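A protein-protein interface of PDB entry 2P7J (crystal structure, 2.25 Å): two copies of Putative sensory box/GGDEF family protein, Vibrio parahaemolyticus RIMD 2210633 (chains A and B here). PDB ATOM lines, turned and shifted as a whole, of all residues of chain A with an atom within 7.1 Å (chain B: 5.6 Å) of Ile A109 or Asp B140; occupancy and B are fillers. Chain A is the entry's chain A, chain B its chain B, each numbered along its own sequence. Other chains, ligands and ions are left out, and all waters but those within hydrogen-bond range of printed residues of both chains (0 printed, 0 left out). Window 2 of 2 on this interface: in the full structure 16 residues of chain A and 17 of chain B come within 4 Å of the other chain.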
ATOM      1  N   GLN A  81      26.522  10.769 -10.871  1.00  0.00           N
ATOM      2  CA  GLN A  81      26.988   9.846 -11.917  1.00  0.00           C
ATOM      3  C   GLN A  81      28.151  10.498 -12.631  1.00  0.00           C
ATOM      4  O   GLN A  81      28.241  11.735 -12.673  1.00  0.00           O
ATOM      5  CB  GLN A  81      25.902   9.546 -12.960  1.00  0.00           C
ATOM      6  CG  GLN A  81      24.609   8.911 -12.462  1.00  0.00           C
ATOM      7  CD  GLN A  81      23.608   8.675 -13.596  1.00  0.00           C
ATOM      8  OE1 GLN A  81      22.595   9.388 -13.731  1.00  0.00           O
ATOM      9  NE2 GLN A  81      23.901   7.689 -14.428  1.00  0.00           N
ATOM     10  N   GLU A  91      25.466   4.629 -23.309  1.00  0.00           N
ATOM     11  CA  GLU A  91      26.412   4.697 -22.187  1.00  0.00           C
ATOM     12  C   GLU A  91      27.401   3.541 -22.328  1.00  0.00           C
ATOM     13  O   GLU A  91      26.981   2.406 -22.555  1.00  0.00           O
ATOM     14  CB  GLU A  91      25.679   4.589 -20.842  1.00  0.00           C
ATOM     15  CG  GLU A  91      24.598   5.660 -20.608  1.00  0.00           C
ATOM     16  CD  GLU A  91      23.714   5.366 -19.390  1.00  0.00           C
ATOM     17  OE1 GLU A  91      23.319   4.204 -19.159  1.00  0.00           O
ATOM     18  OE2 GLU A  91      23.368   6.315 -18.665  1.00  0.00           O
ATOM     19  N   ARG A  94      29.728   3.874 -16.739  1.00  0.00           N
ATOM     20  CA  ARG A  94      28.798   4.506 -15.808  1.00  0.00           C
ATOM     21  C   ARG A  94      29.188   4.227 -14.339  1.00  0.00           C
ATOM     22  O   ARG A  94      29.130   3.092 -13.877  1.00  0.00           O
ATOM     23  CB  ARG A  94      27.379   4.043 -16.121  1.00  0.00           C
ATOM     24  CG  ARG A  94      26.326   4.629 -15.222  1.00  0.00           C
ATOM     25  CD  ARG A  94      24.912   4.197 -15.617  1.00  0.00           C
ATOM     26  NE  ARG A  94      23.990   4.843 -14.681  1.00  0.00           N
ATOM     27  CZ  ARG A  94      22.843   4.328 -14.255  1.00  0.00           C
ATOM     28  NH1 ARG A  94      22.436   3.151 -14.700  1.00  0.00           N
ATOM     29  NH2 ARG A  94      22.104   4.994 -13.384  1.00  0.00           N
ATOM     30  N   LYS A  96      28.037   5.238 -10.508  1.00  0.00           N
ATOM     31  CA  LYS A  96      27.034   5.860  -9.650  1.00  0.00           C
ATOM     32  C   LYS A  96      27.647   6.182  -8.288  1.00  0.00           C
ATOM     33  O   LYS A  96      28.483   5.421  -7.776  1.00  0.00           O
ATOM     34  CB  LYS A  96      25.812   4.942  -9.457  1.00  0.00           C
ATOM     35  CG  LYS A  96      25.008   4.684 -10.714  1.00  0.00           C
ATOM     36  CD  LYS A  96      24.188   3.400 -10.572  1.00  0.00           C
ATOM     37  CE  LYS A  96      22.858   3.656  -9.892  1.00  0.00           C
ATOM     38  NZ  LYS A  96      22.915   3.280  -8.434  1.00  0.00           N
ATOM     39  N   PRO A 106      30.848   1.166 -10.353  1.00  0.00           N
ATOM     40  CA  PRO A 106      30.332   1.010 -11.735  1.00  0.00           C
ATOM     41  C   PRO A 106      28.959   0.354 -11.801  1.00  0.00           C
ATOM     42  O   PRO A 106      28.637  -0.497 -10.971  1.00  0.00           O
ATOM     43  CB  PRO A 106      31.316   0.038 -12.371  1.00  0.00           C
ATOM     44  CG  PRO A 106      31.871  -0.766 -11.181  1.00  0.00           C
ATOM     45  CD  PRO A 106      32.010   0.291 -10.094  1.00  0.00           C
ATOM     46  N   SER A 107      28.170   0.737 -12.799  1.00  0.00           N
ATOM     47  CA  SER A 107      26.965   0.002 -13.161  1.00  0.00           C
ATOM     48  C   SER A 107      27.108  -0.655 -14.548  1.00  0.00           C
ATOM     49  O   SER A 107      27.777  -0.129 -15.454  1.00  0.00           O
ATOM     50  CB  SER A 107      25.759   0.927 -13.111  1.00  0.00           C
ATOM     51  OG  SER A 107      24.574   0.246 -13.495  1.00  0.00           O
ATOM     52  N   LEU A 108      26.469  -1.810 -14.697  1.00  0.00           N
ATOM     53  CA  LEU A 108      26.373  -2.488 -15.986  1.00  0.00           C
ATOM     54  C   LEU A 108      25.021  -2.228 -16.635  1.00  0.00           C
ATOM     55  O   LEU A 108      24.711  -2.767 -17.694  1.00  0.00           O
ATOM     56  CB  LEU A 108      26.668  -3.993 -15.837  1.00  0.00           C
ATOM     57  CG  LEU A 108      28.135  -4.271 -15.421  1.00  0.00           C
ATOM     58  CD1 LEU A 108      28.300  -5.683 -14.883  1.00  0.00           C
ATOM     59  CD2 LEU A 108      29.110  -4.036 -16.582  1.00  0.00           C
ATOM     60  N   ILE A 109      24.226  -1.363 -16.014  1.00  0.00           N
ATOM     61  CA  ILE A 109      22.944  -0.972 -16.570  1.00  0.00           C
ATOM     62  C   ILE A 109      23.244   0.210 -17.454  1.00  0.00           C
ATOM     63  O   ILE A 109      23.299   1.347 -16.996  1.00  0.00           O
ATOM     64  CB  ILE A 109      21.899  -0.660 -15.443  1.00  0.00           C
ATOM     65  CG1 ILE A 109      21.616  -1.930 -14.648  1.00  0.00           C
ATOM     66  CG2 ILE A 109      20.599  -0.111 -16.005  1.00  0.00           C
ATOM     67  CD1 ILE A 109      20.894  -1.656 -13.335  1.00  0.00           C
ATOM     68  N   LEU A 110      23.481  -0.105 -18.725  1.00  0.00           N
ATOM     69  CA  LEU A 110      23.935   0.850 -19.719  1.00  0.00           C
ATOM     70  C   LEU A 110      22.869   1.042 -20.804  1.00  0.00           C
ATOM     71  O   LEU A 110      22.412   0.069 -21.420  1.00  0.00           O
ATOM     72  CB  LEU A 110      25.277   0.401 -20.313  1.00  0.00           C
ATOM     73  CG  LEU A 110      26.417   0.314 -19.291  1.00  0.00           C
ATOM     74  CD1 LEU A 110      27.596  -0.500 -19.851  1.00  0.00           C
ATOM     75  CD2 LEU A 110      26.898   1.685 -18.758  1.00  0.00           C
ATOM     76  N   ARG A 111      22.498   2.300 -21.034  1.00  0.00           N
ATOM     77  CA  ARG A 111      21.342   2.660 -21.851  1.00  0.00           C
ATOM     78  C   ARG A 111      21.679   3.467 -23.097  1.00  0.00           C
ATOM     79  O   ARG A 111      22.730   4.116 -23.179  1.00  0.00           O
ATOM     80  CB  ARG A 111      20.352   3.500 -21.028  1.00  0.00           C
ATOM     81  CG  ARG A 111      19.751   2.830 -19.811  1.00  0.00           C
ATOM     82  CD  ARG A 111      18.869   1.625 -20.174  1.00  0.00           C
ATOM     83  NE  ARG A 111      18.132   1.158 -19.002  1.00  0.00           N
ATOM     84  CZ  ARG A 111      17.839  -0.114 -18.729  1.00  0.00           C
ATOM     85  NH1 ARG A 111      18.217  -1.095 -19.520  1.00  0.00           N
ATOM     86  NH2 ARG A 111      17.176  -0.394 -17.633  1.00  0.00           N
ATOM     87  N   ASP A 140      15.234   7.058 -16.410  1.00  0.00           N
ATOM     88  CA  ASP A 140      15.668   5.721 -16.777  1.00  0.00           C
ATOM     89  C   ASP A 140      14.669   5.204 -17.801  1.00  0.00           C
ATOM     90  O   ASP A 140      13.484   5.029 -17.487  1.00  0.00           O
ATOM     91  CB  ASP A 140      15.716   4.802 -15.549  1.00  0.00           C
ATOM     92  CG  ASP A 140      16.389   3.474 -15.844  1.00  0.00           C
ATOM     93  OD1 ASP A 140      17.175   3.401 -16.818  1.00  0.00           O
ATOM     94  OD2 ASP A 140      16.155   2.497 -15.104  1.00  0.00           O
ATOM     95  N   ILE B 109       9.802  -0.780 -17.307  1.00  0.00           N
ATOM     96  CA  ILE B 109      11.071  -1.412 -16.996  1.00  0.00           C
ATOM     97  C   ILE B 109      10.840  -2.726 -16.230  1.00  0.00           C
ATOM     98  O   ILE B 109      10.677  -2.730 -14.992  1.00  0.00           O
ATOM     99  CB  ILE B 109      12.013  -0.463 -16.205  1.00  0.00           C
ATOM    100  CG1 ILE B 109      12.315   0.800 -17.016  1.00  0.00           C
ATOM    101  CG2 ILE B 109      13.315  -1.171 -15.876  1.00  0.00           C
ATOM    102  CD1 ILE B 109      13.052   1.885 -16.231  1.00  0.00           C
ATOM    103  N   ARG B 111      11.871  -6.827 -15.615  1.00  0.00           N
ATOM    104  CA  ARG B 111      13.037  -7.676 -15.550  1.00  0.00           C
ATOM    105  C   ARG B 111      12.716  -9.138 -15.212  1.00  0.00           C
ATOM    106  O   ARG B 111      11.665  -9.472 -14.616  1.00  0.00           O
ATOM    107  CB  ARG B 111      14.031  -7.151 -14.501  1.00  0.00           C
ATOM    108  CG  ARG B 111      14.316  -5.667 -14.542  1.00  0.00           C
ATOM    109  CD  ARG B 111      15.404  -5.317 -15.572  1.00  0.00           C
ATOM    110  NE  ARG B 111      16.056  -4.091 -15.165  1.00  0.00           N
ATOM    111  CZ  ARG B 111      16.489  -3.133 -15.973  1.00  0.00           C
ATOM    112  NH1 ARG B 111      16.343  -3.229 -17.279  1.00  0.00           N
ATOM    113  NH2 ARG B 111      17.049  -2.057 -15.444  1.00  0.00           N
ATOM    114  N   LYS B 113      13.381 -11.786 -12.750  1.00  0.00           N
ATOM    115  CA  LYS B 113      13.741 -11.818 -11.312  1.00  0.00           C
ATOM    116  C   LYS B 113      13.968 -13.225 -10.743  1.00  0.00           C
ATOM    117  O   LYS B 113      14.048 -13.392  -9.510  1.00  0.00           O
ATOM    118  CB  LYS B 113      12.693 -11.051 -10.454  1.00  0.00           C
ATOM    119  CG  LYS B 113      12.624  -9.562 -10.750  1.00  0.00           C
ATOM    120  CD  LYS B 113      13.795  -8.831 -10.123  1.00  0.00           C
ATOM    121  CE  LYS B 113      13.739  -7.325 -10.411  1.00  0.00           C
ATOM    122  NZ  LYS B 113      14.571  -6.558  -9.419  1.00  0.00           N
ATOM    123  N   ARG B 116      16.575 -14.355  -8.031  1.00  0.00           N
ATOM    124  CA  ARG B 116      16.420 -13.826  -6.672  1.00  0.00           C
ATOM    125  C   ARG B 116      15.824 -14.863  -5.703  1.00  0.00           C
ATOM    126  O   ARG B 116      14.922 -15.648  -6.064  1.00  0.00           O
ATOM    127  CB  ARG B 116      15.555 -12.557  -6.678  1.00  0.00           C
ATOM    128  CG  ARG B 116      16.126 -11.372  -7.471  1.00  0.00           C
ATOM    129  CD  ARG B 116      17.392 -10.773  -6.810  1.00  0.00           C
ATOM    130  NE  ARG B 116      17.125 -10.116  -5.537  1.00  0.00           N
ATOM    131  CZ  ARG B 116      16.549  -8.918  -5.398  1.00  0.00           C
ATOM    132  NH1 ARG B 116      16.159  -8.223  -6.453  1.00  0.00           N
ATOM    133  NH2 ARG B 116      16.349  -8.411  -4.187  1.00  0.00           N
ATOM    134  N   GLU B 138      16.645  -3.705  -2.043  1.00  0.00           N
ATOM    135  CA  GLU B 138      16.202  -3.790  -3.428  1.00  0.00           C
ATOM    136  C   GLU B 138      17.375  -3.729  -4.417  1.00  0.00           C
ATOM    137  O   GLU B 138      18.406  -3.108  -4.145  1.00  0.00           O
ATOM    138  CB  GLU B 138      15.207  -2.688  -3.745  1.00  0.00           C
ATOM    139  CG  GLU B 138      13.824  -2.976  -3.258  1.00  0.00           C
ATOM    140  CD  GLU B 138      12.895  -1.835  -3.507  1.00  0.00           C
ATOM    141  OE1 GLU B 138      13.372  -0.792  -4.023  1.00  0.00           O
ATOM    142  OE2 GLU B 138      11.689  -1.976  -3.199  1.00  0.00           O
ATOM    143  N   ARG B 139      17.183  -4.380  -5.563  1.00  0.00           N
ATOM    144  CA  ARG B 139      18.185  -4.486  -6.613  1.00  0.00           C
ATOM    145  C   ARG B 139      17.539  -4.332  -7.988  1.00  0.00           C
ATOM    146  O   ARG B 139      16.332  -4.611  -8.148  1.00  0.00           O
ATOM    147  CB  ARG B 139      18.872  -5.844  -6.541  1.00  0.00           C
ATOM    148  CG  ARG B 139      19.807  -5.991  -5.359  1.00  0.00           C
ATOM    149  CD  ARG B 139      20.393  -7.405  -5.243  1.00  0.00           C
ATOM    150  NE  ARG B 139      21.142  -7.483  -3.999  1.00  0.00           N
ATOM    151  CZ  ARG B 139      22.451  -7.245  -3.879  1.00  0.00           C
ATOM    152  NH1 ARG B 139      23.211  -6.959  -4.959  1.00  0.00           N
ATOM    153  NH2 ARG B 139      23.006  -7.311  -2.666  1.00  0.00           N
ATOM    154  N   ASP B 140      18.338  -3.876  -8.960  1.00  0.00           N
ATOM    155  CA  ASP B 140      17.981  -3.846 -10.383  1.00  0.00           C
ATOM    156  C   ASP B 140      19.131  -4.532 -11.096  1.00  0.00           C
ATOM    157  O   ASP B 140      20.292  -4.143 -10.940  1.00  0.00           O
ATOM    158  CB  ASP B 140      17.797  -2.402 -10.911  1.00  0.00           C
ATOM    159  CG  ASP B 140      17.099  -2.339 -12.301  1.00  0.00           C
ATOM    160  OD1 ASP B 140      16.346  -3.253 -12.688  1.00  0.00           O
ATOM    161  OD2 ASP B 140      17.277  -1.338 -13.025  1.00  0.00           O
ATOM    162  N   LYS B 141      18.798  -5.569 -11.860  1.00  0.00           N
ATOM    163  CA  LYS B 141      19.783  -6.435 -12.531  1.00  0.00           C
ATOM    164  C   LYS B 141      20.940  -6.886 -11.624  1.00  0.00           C
ATOM    165  O   LYS B 141      22.129  -6.866 -12.010  1.00  0.00           O
ATOM    166  CB  LYS B 141      20.274  -5.782 -13.817  1.00  0.00           C
ATOM    167  CG  LYS B 141      19.128  -5.550 -14.782  1.00  0.00           C
ATOM    168  CD  LYS B 141      19.637  -5.303 -16.190  1.00  0.00           C
ATOM    169  CE  LYS B 141      19.967  -6.598 -16.926  1.00  0.00           C
ATOM    170  NZ  LYS B 141      20.712  -6.295 -18.200  1.00  0.00           N
ATOM    171  N   GLY B 142      20.567  -7.295 -10.408  1.00  0.00           N
ATOM    172  CA  GLY B 142      21.516  -7.789  -9.421  1.00  0.00           C
ATOM    173  C   GLY B 142      22.282  -6.692  -8.733  1.00  0.00           C
ATOM    174  O   GLY B 142      23.086  -6.978  -7.843  1.00  0.00           O
ATOM    175  N   GLU B 143      22.034  -5.437  -9.116  1.00  0.00           N
ATOM    176  CA  GLU B 143      22.754  -4.297  -8.546  1.00  0.00           C
ATOM    177  C   GLU B 143      21.907  -3.569  -7.540  1.00  0.00           C
ATOM    178  O   GLU B 143      20.729  -3.341  -7.744  1.00  0.00           O
ATOM    179  CB  GLU B 143      23.194  -3.297  -9.631  1.00  0.00           C
ATOM    180  CG  GLU B 143      24.145  -3.866 -10.692  1.00  0.00           C
ATOM    181  CD  GLU B 143      24.528  -2.827 -11.770  1.00  0.00           C
ATOM    182  OE1 GLU B 143      24.136  -1.645 -11.666  1.00  0.00           O
ATOM    183  OE2 GLU B 143      25.236  -3.205 -12.734  1.00  0.00           O
ATOM    184  N   LEU B 144      22.526  -3.157  -6.458  1.00  0.00           N
ATOM    185  CA  LEU B 144      21.818  -2.464  -5.404  1.00  0.00           C
ATOM    186  C   LEU B 144      21.221  -1.171  -5.908  1.00  0.00           C
ATOM    187  O   LEU B 144      21.862  -0.417  -6.648  1.00  0.00           O
ATOM    188  CB  LEU B 144      22.784  -2.186  -4.241  1.00  0.00           C
ATOM    189  CG  LEU B 144      23.134  -3.359  -3.338  1.00  0.00           C
ATOM    190  CD1 LEU B 144      24.260  -2.968  -2.407  1.00  0.00           C
ATOM    191  CD2 LEU B 144      21.891  -3.757  -2.532  1.00  0.00           C
ATOM    192  N   VAL B 145      19.985  -0.914  -5.501  1.00  0.00           N
ATOM    193  CA  VAL B 145      19.344   0.355  -5.784  1.00  0.00           C
ATOM    194  C   VAL B 145      19.796   1.357  -4.715  1.00  0.00           C
ATOM    195  O   VAL B 145      19.919   0.995  -3.553  1.00  0.00           O
ATOM    196  CB  VAL B 145      17.805   0.225  -5.787  1.00  0.00           C
ATOM    197  CG1 VAL B 145      17.148   1.599  -5.947  1.00  0.00           C
ATOM    198  CG2 VAL B 145      17.336  -0.717  -6.898  1.00  0.00           C
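NH2 of Arg A111 lies close to NH2 of Arg B111.
OE1 of Glu B143 lies within hydrogen-bond range of OG of Ser A107, at 2.7 Å.
The side-chain carboxylate (OE2) of Glu B143 is in hydrogen-bond range of the backbone NH (N) of Leu A108, 2.7 Å away.
The backbone carbonyl oxygen of Arg A94 lies within hydrogen-bond range of the backbone NH of Ser A107 (2.8 Å).
The side-chain hydroxyl (OG) of Ser A107 lies within hydrogen-bond range of the backbone NH (N) of Ile A109 (3.0 Å).
O of Ile A109 lies within hydrogen-bond range of NH1 of Arg A94, at 3.0 Å.
The guanidinium group of Arg B111 is in salt-bridge range of the side-chain carboxylate of Asp B140 (2.5 Å).
The guanidinium group (NE) of Arg A111 is in salt-bridge range of the side-chain carboxylate (OD1) of Asp A140.
N of Glu A91 is in hydrogen-bond range of O of Arg A111 (2.8 Å).
Asp B140 touches Ile A109 (O to CD1, 3.5 Å).
Ile A109 touches Glu B143 (CD1 to OE1, 3.6 Å).
CD1 of Ile B109 touches OD2 of Asp A140, 3.4 Å away.
Of the printed residues of chain B, Ile A109 touches Asp B140 and Glu B143.
Printed residues of chain B within 4 Å of Asp A140: Ile B109.
Of the printed residues of chain A, Asp B140 touches Ile A109.
Printed residues of chain A within 4 Å of Glu B143: Ser A107 (2.7 Å), Leu A108 (2.7 Å) and Ile A109 (3.6 Å).
The nearest printed residue of chain B that does not touch Ile A109 is Arg B111 (4.1 Å).
The nearest printed residue of chain B that does not touch Arg A111 is Ile B109 (4.3 Å).
Of the 12 printed residues of chain B, 4 touch a printed residue of chain A.
Among the printed residues, 6 pairs touch across the chains.
Among the printed residues, no Asp or Glu carboxylate lies within 4 Å of a Lys or Arg side-chain nitrogen of the other chain.
Ile A109 touches Asp B140, and with the chains exchanged Asp A140 touches Ile B109.
Arg B111 touches its own counterpart, Arg A111.
Positions printed for both chains: 109, 111 and 140.
Of the 6 pairs that touch across the chains among the printed residues, 3 have their exchanged pair printed and touching as well.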
